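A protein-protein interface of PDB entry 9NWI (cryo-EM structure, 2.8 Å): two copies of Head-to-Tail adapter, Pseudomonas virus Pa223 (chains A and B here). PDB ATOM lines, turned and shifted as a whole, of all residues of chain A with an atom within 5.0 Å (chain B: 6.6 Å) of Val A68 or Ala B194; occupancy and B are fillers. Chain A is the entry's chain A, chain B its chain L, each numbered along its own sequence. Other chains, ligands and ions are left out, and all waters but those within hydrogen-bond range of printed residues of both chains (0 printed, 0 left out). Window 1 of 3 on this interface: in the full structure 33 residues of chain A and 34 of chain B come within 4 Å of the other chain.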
ATOM      1  N   ASN A  40       5.452   9.002  23.313  1.00  0.00           N
ATOM      2  CA  ASN A  40       6.868   8.795  23.602  1.00  0.00           C
ATOM      3  C   ASN A  40       7.168   7.371  24.044  1.00  0.00           C
ATOM      4  O   ASN A  40       8.314   6.924  23.926  1.00  0.00           O
ATOM      5  CB  ASN A  40       7.333   9.770  24.680  1.00  0.00           C
ATOM      6  CG  ASN A  40       7.914  11.037  24.104  1.00  0.00           C
ATOM      7  OD1 ASN A  40       8.305  11.080  22.940  1.00  0.00           O
ATOM      8  ND2 ASN A  40       7.971  12.082  24.917  1.00  0.00           N
ATOM      9  N   ARG A  44       8.989   4.336  17.580  1.00  0.00           N
ATOM     10  CA  ARG A  44      10.414   4.223  17.255  1.00  0.00           C
ATOM     11  C   ARG A  44      10.503   4.244  15.730  1.00  0.00           C
ATOM     12  O   ARG A  44      10.386   3.202  15.079  1.00  0.00           O
ATOM     13  CB  ARG A  44      11.035   2.958  17.835  1.00  0.00           C
ATOM     14  CG  ARG A  44      10.688   2.681  19.284  1.00  0.00           C
ATOM     15  CD  ARG A  44      11.619   3.419  20.221  1.00  0.00           C
ATOM     16  NE  ARG A  44      11.322   3.128  21.616  1.00  0.00           N
ATOM     17  CZ  ARG A  44      10.465   3.815  22.357  1.00  0.00           C
ATOM     18  NH1 ARG A  44       9.797   4.845  21.863  1.00  0.00           N
ATOM     19  NH2 ARG A  44      10.270   3.460  23.622  1.00  0.00           N
ATOM     20  N   HIS A  66      17.956  12.856  26.608  1.00  0.00           N
ATOM     21  CA  HIS A  66      16.726  12.550  25.892  1.00  0.00           C
ATOM     22  C   HIS A  66      16.656  11.098  25.446  1.00  0.00           C
ATOM     23  O   HIS A  66      15.745  10.733  24.699  1.00  0.00           O
ATOM     24  CB  HIS A  66      16.577  13.474  24.683  1.00  0.00           C
ATOM     25  CG  HIS A  66      16.248  14.888  25.044  1.00  0.00           C
ATOM     26  ND1 HIS A  66      15.694  15.235  26.258  1.00  0.00           N
ATOM     27  CD2 HIS A  66      16.394  16.042  24.353  1.00  0.00           C
ATOM     28  CE1 HIS A  66      15.514  16.543  26.298  1.00  0.00           C
ATOM     29  NE2 HIS A  66      15.930  17.056  25.155  1.00  0.00           N
ATOM     30  N   PHE A  67      17.603  10.273  25.881  1.00  0.00           N
ATOM     31  CA  PHE A  67      17.658   8.883  25.456  1.00  0.00           C
ATOM     32  C   PHE A  67      16.425   8.121  25.918  1.00  0.00           C
ATOM     33  O   PHE A  67      15.966   8.277  27.052  1.00  0.00           O
ATOM     34  CB  PHE A  67      18.925   8.235  26.014  1.00  0.00           C
ATOM     35  CG  PHE A  67      18.979   6.751  25.848  1.00  0.00           C
ATOM     36  CD1 PHE A  67      19.508   6.195  24.702  1.00  0.00           C
ATOM     37  CD2 PHE A  67      18.525   5.910  26.846  1.00  0.00           C
ATOM     38  CE1 PHE A  67      19.571   4.835  24.549  1.00  0.00           C
ATOM     39  CE2 PHE A  67      18.582   4.545  26.693  1.00  0.00           C
ATOM     40  CZ  PHE A  67      19.106   4.007  25.543  1.00  0.00           C
ATOM     41  N   VAL A  68      15.878   7.295  25.024  1.00  0.00           N
ATOM     42  CA  VAL A  68      14.783   6.395  25.353  1.00  0.00           C
ATOM     43  C   VAL A  68      15.120   4.945  25.026  1.00  0.00           C
ATOM     44  O   VAL A  68      14.883   4.052  25.845  1.00  0.00           O
ATOM     45  CB  VAL A  68      13.473   6.824  24.656  1.00  0.00           C
ATOM     46  CG1 VAL A  68      13.699   7.076  23.185  1.00  0.00           C
ATOM     47  CG2 VAL A  68      12.405   5.772  24.847  1.00  0.00           C
ATOM     48  N   ALA A  69      15.677   4.687  23.844  1.00  0.00           N
ATOM     49  CA  ALA A  69      16.079   3.346  23.448  1.00  0.00           C
ATOM     50  C   ALA A  69      17.359   3.429  22.631  1.00  0.00           C
ATOM     51  O   ALA A  69      17.604   4.416  21.935  1.00  0.00           O
ATOM     52  CB  ALA A  69      14.985   2.641  22.641  1.00  0.00           C
ATOM     53  N   LEU A  70      18.173   2.382  22.721  1.00  0.00           N
ATOM     54  CA  LEU A  70      19.483   2.350  22.086  1.00  0.00           C
ATOM     55  C   LEU A  70      19.446   1.466  20.849  1.00  0.00           C
ATOM     56  O   LEU A  70      18.915   0.352  20.891  1.00  0.00           O
ATOM     57  CB  LEU A  70      20.548   1.837  23.055  1.00  0.00           C
ATOM     58  CG  LEU A  70      21.899   1.505  22.424  1.00  0.00           C
ATOM     59  CD1 LEU A  70      22.651   2.776  22.089  1.00  0.00           C
ATOM     60  CD2 LEU A  70      22.719   0.625  23.344  1.00  0.00           C
ATOM     61  N   TRP A 132      17.313   6.365  19.816  1.00  0.00           N
ATOM     62  CA  TRP A 132      16.060   7.087  19.669  1.00  0.00           C
ATOM     63  C   TRP A 132      15.901   8.095  20.799  1.00  0.00           C
ATOM     64  O   TRP A 132      16.484   7.943  21.875  1.00  0.00           O
ATOM     65  CB  TRP A 132      14.877   6.121  19.658  1.00  0.00           C
ATOM     66  CG  TRP A 132      14.719   5.393  18.365  1.00  0.00           C
ATOM     67  CD1 TRP A 132      14.201   5.885  17.207  1.00  0.00           C
ATOM     68  CD2 TRP A 132      15.090   4.038  18.094  1.00  0.00           C
ATOM     69  NE1 TRP A 132      14.221   4.922  16.232  1.00  0.00           N
ATOM     70  CE2 TRP A 132      14.763   3.777  16.752  1.00  0.00           C
ATOM     71  CE3 TRP A 132      15.666   3.019  18.856  1.00  0.00           C
ATOM     72  CZ2 TRP A 132      14.992   2.543  16.155  1.00  0.00           C
ATOM     73  CZ3 TRP A 132      15.891   1.796  18.263  1.00  0.00           C
ATOM     74  CH2 TRP A 132      15.556   1.568  16.926  1.00  0.00           C
ATOM     75  N   THR A 133      15.110   9.130  20.545  1.00  0.00           N
ATOM     76  CA  THR A 133      14.864  10.194  21.510  1.00  0.00           C
ATOM     77  C   THR A 133      13.364  10.316  21.772  1.00  0.00           C
ATOM     78  O   THR A 133      12.561   9.501  21.313  1.00  0.00           O
ATOM     79  CB  THR A 133      15.443  11.520  21.018  1.00  0.00           C
ATOM     80  OG1 THR A 133      14.922  11.815  19.717  1.00  0.00           O
ATOM     81  CG2 THR A 133      16.952  11.447  20.946  1.00  0.00           C
ATOM     82  N   VAL A 134      12.993  11.346  22.519  1.00  0.00           N
ATOM     83  CA  VAL A 134      11.594  11.631  22.791  1.00  0.00           C
ATOM     84  C   VAL A 134      11.078  12.610  21.746  1.00  0.00           C
ATOM     85  O   VAL A 134      11.836  13.358  21.126  1.00  0.00           O
ATOM     86  CB  VAL A 134      11.392  12.183  24.214  1.00  0.00           C
ATOM     87  CG1 VAL A 134      11.752  11.133  25.243  1.00  0.00           C
ATOM     88  CG2 VAL A 134      12.223  13.434  24.414  1.00  0.00           C
ATOM     89  N   ARG B  46      15.920   2.954  35.862  1.00  0.00           N
ATOM     90  CA  ARG B  46      17.245   3.547  36.009  1.00  0.00           C
ATOM     91  C   ARG B  46      17.266   4.607  37.101  1.00  0.00           C
ATOM     92  O   ARG B  46      18.207   4.662  37.900  1.00  0.00           O
ATOM     93  CB  ARG B  46      17.700   4.146  34.681  1.00  0.00           C
ATOM     94  CG  ARG B  46      18.524   3.207  33.830  1.00  0.00           C
ATOM     95  CD  ARG B  46      18.984   3.889  32.557  1.00  0.00           C
ATOM     96  NE  ARG B  46      17.933   3.912  31.548  1.00  0.00           N
ATOM     97  CZ  ARG B  46      17.407   5.020  31.045  1.00  0.00           C
ATOM     98  NH1 ARG B  46      17.815   6.217  31.433  1.00  0.00           N
ATOM     99  NH2 ARG B  46      16.446   4.924  30.132  1.00  0.00           N
ATOM    100  N   LYS B 150       8.723  12.365  34.624  1.00  0.00           N
ATOM    101  CA  LYS B 150       8.854  11.333  33.600  1.00  0.00           C
ATOM    102  C   LYS B 150       7.512  10.992  32.963  1.00  0.00           C
ATOM    103  O   LYS B 150       7.419  10.834  31.741  1.00  0.00           O
ATOM    104  CB  LYS B 150       9.491  10.081  34.199  1.00  0.00           C
ATOM    105  CG  LYS B 150      10.116   9.158  33.173  1.00  0.00           C
ATOM    106  CD  LYS B 150      11.508   9.622  32.791  1.00  0.00           C
ATOM    107  CE  LYS B 150      12.370   8.454  32.350  1.00  0.00           C
ATOM    108  NZ  LYS B 150      11.970   7.947  31.010  1.00  0.00           N
ATOM    109  N   ASN B 189       7.879  -1.623  30.741  1.00  0.00           N
ATOM    110  CA  ASN B 189       8.311  -2.337  29.545  1.00  0.00           C
ATOM    111  C   ASN B 189       9.300  -1.509  28.738  1.00  0.00           C
ATOM    112  O   ASN B 189      10.293  -2.043  28.224  1.00  0.00           O
ATOM    113  CB  ASN B 189       7.102  -2.710  28.692  1.00  0.00           C
ATOM    114  CG  ASN B 189       7.495  -3.221  27.325  1.00  0.00           C
ATOM    115  OD1 ASN B 189       7.677  -2.445  26.387  1.00  0.00           O
ATOM    116  ND2 ASN B 189       7.629  -4.534  27.202  1.00  0.00           N
ATOM    117  N   GLU B 190       9.043  -0.206  28.605  1.00  0.00           N
ATOM    118  CA  GLU B 190       9.983   0.638  27.876  1.00  0.00           C
ATOM    119  C   GLU B 190      11.337   0.665  28.562  1.00  0.00           C
ATOM    120  O   GLU B 190      12.380   0.617  27.899  1.00  0.00           O
ATOM    121  CB  GLU B 190       9.441   2.057  27.733  1.00  0.00           C
ATOM    122  CG  GLU B 190      10.437   2.996  27.074  1.00  0.00           C
ATOM    123  CD  GLU B 190      10.208   4.448  27.425  1.00  0.00           C
ATOM    124  OE1 GLU B 190      10.491   4.836  28.576  1.00  0.00           O
ATOM    125  OE2 GLU B 190       9.753   5.205  26.543  1.00  0.00           O
ATOM    126  N   GLU B 191      11.347   0.744  29.894  1.00  0.00           N
ATOM    127  CA  GLU B 191      12.620   0.726  30.607  1.00  0.00           C
ATOM    128  C   GLU B 191      13.333  -0.609  30.435  1.00  0.00           C
ATOM    129  O   GLU B 191      14.559  -0.653  30.289  1.00  0.00           O
ATOM    130  CB  GLU B 191      12.402   1.026  32.086  1.00  0.00           C
ATOM    131  CG  GLU B 191      13.542   1.792  32.720  1.00  0.00           C
ATOM    132  CD  GLU B 191      13.440   3.284  32.482  1.00  0.00           C
ATOM    133  OE1 GLU B 191      12.473   3.717  31.823  1.00  0.00           O
ATOM    134  OE2 GLU B 191      14.325   4.024  32.957  1.00  0.00           O
ATOM    135  N   ASN B 192      12.580  -1.712  30.458  1.00  0.00           N
ATOM    136  CA  ASN B 192      13.189  -3.031  30.323  1.00  0.00           C
ATOM    137  C   ASN B 192      13.816  -3.219  28.950  1.00  0.00           C
ATOM    138  O   ASN B 192      14.914  -3.773  28.831  1.00  0.00           O
ATOM    139  CB  ASN B 192      12.148  -4.118  30.578  1.00  0.00           C
ATOM    140  CG  ASN B 192      11.872  -4.326  32.046  1.00  0.00           C
ATOM    141  OD1 ASN B 192      12.550  -3.762  32.902  1.00  0.00           O
ATOM    142  ND2 ASN B 192      10.872  -5.145  32.349  1.00  0.00           N
ATOM    143  N   ALA B 193      13.136  -2.762  27.899  1.00  0.00           N
ATOM    144  CA  ALA B 193      13.570  -3.020  26.531  1.00  0.00           C
ATOM    145  C   ALA B 193      14.464  -1.921  25.974  1.00  0.00           C
ATOM    146  O   ALA B 193      14.449  -1.673  24.763  1.00  0.00           O
ATOM    147  CB  ALA B 193      12.356  -3.223  25.626  1.00  0.00           C
ATOM    148  N   ALA B 194      15.242  -1.250  26.820  1.00  0.00           N
ATOM    149  CA  ALA B 194      16.029  -0.106  26.390  1.00  0.00           C
ATOM    150  C   ALA B 194      17.521  -0.378  26.288  1.00  0.00           C
ATOM    151  O   ALA B 194      18.241   0.445  25.715  1.00  0.00           O
ATOM    152  CB  ALA B 194      15.806   1.078  27.342  1.00  0.00           C
ATOM    153  N   ASP B 195      18.009  -1.499  26.817  1.00  0.00           N
ATOM    154  CA  ASP B 195      19.444  -1.753  26.886  1.00  0.00           C
ATOM    155  C   ASP B 195      19.947  -2.595  25.719  1.00  0.00           C
ATOM    156  O   ASP B 195      20.870  -2.187  25.009  1.00  0.00           O
ATOM    157  CB  ASP B 195      19.791  -2.425  28.219  1.00  0.00           C
ATOM    158  CG  ASP B 195      20.069  -1.422  29.314  1.00  0.00           C
ATOM    159  OD1 ASP B 195      20.481  -0.290  28.986  1.00  0.00           O
ATOM    160  OD2 ASP B 195      19.877  -1.762  30.499  1.00  0.00           O
ATOM    161  N   PHE B 196      19.360  -3.775  25.509  1.00  0.00           N
ATOM    162  CA  PHE B 196      19.848  -4.690  24.485  1.00  0.00           C
ATOM    163  C   PHE B 196      18.724  -5.253  23.625  1.00  0.00           C
ATOM    164  O   PHE B 196      18.897  -6.304  23.003  1.00  0.00           O
ATOM    165  CB  PHE B 196      20.640  -5.835  25.119  1.00  0.00           C
ATOM    166  CG  PHE B 196      19.908  -6.538  26.222  1.00  0.00           C
ATOM    167  CD1 PHE B 196      19.027  -7.565  25.942  1.00  0.00           C
ATOM    168  CD2 PHE B 196      20.105  -6.175  27.540  1.00  0.00           C
ATOM    169  CE1 PHE B 196      18.355  -8.213  26.954  1.00  0.00           C
ATOM    170  CE2 PHE B 196      19.435  -6.821  28.556  1.00  0.00           C
ATOM    171  CZ  PHE B 196      18.560  -7.841  28.261  1.00  0.00           C
ATOM    172  N   ALA B 197      17.574  -4.582  23.573  1.00  0.00           N
ATOM    173  CA  ALA B 197      16.468  -5.086  22.773  1.00  0.00           C
ATOM    174  C   ALA B 197      16.713  -4.959  21.278  1.00  0.00           C
ATOM    175  O   ALA B 197      15.976  -5.568  20.496  1.00  0.00           O
ATOM    176  CB  ALA B 197      15.177  -4.359  23.143  1.00  0.00           C
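NH2 of Arg A44 is in salt-bridge range of OE2 of Glu B190. The backbone carbonyl oxygen of Asn A40 sits close to the side-chain carboxylate of Glu B190.
O of Asn A40 sits at hydrogen-bond distance from NH1 of Arg A44, 3.3 Å away. O of Trp A132 lies close to N of Val A68 (3.3 Å).
Among the printed residues, pairs that only touch across the chains: Val A68 with Glu B190 (3.2 Å), Val A68 with Ala B194 (3.5 Å), Leu A70 with Ala B194 (3.6 Å), Phe A67 with Ala B194 (3.7 Å) and Leu A70 with Asp B195 (3.8 Å).
Val A68 touches two residues of chain B. Of chain A, only Phe A67, Val A68 and Leu A70 come within 4 Å of Ala B194. Of the printed residues of chain B, Asn A40 touches Glu B190 (3.4 Å). Of the printed residues of chain B, Leu A70 touches Ala B194 and Asp B195. Printed residues of chain B within 4 Å of Arg A44: Glu B190 (3.4 Å). Thr A133 touches none of the printed residues of chain B. Trp A132 touches none of the printed residues of chain B. The nearest printed residue of chain A that does not touch Glu B190 is Ala A69 (6.2 Å).
Hydrophobic or aromatic side chains of chain A within 4 Å of the printed part of chain B: Phe A67, Val A68 and Leu A70. Of the 11 printed residues of chain B, 3 touch a printed residue of chain A.
No position is printed for both chains.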
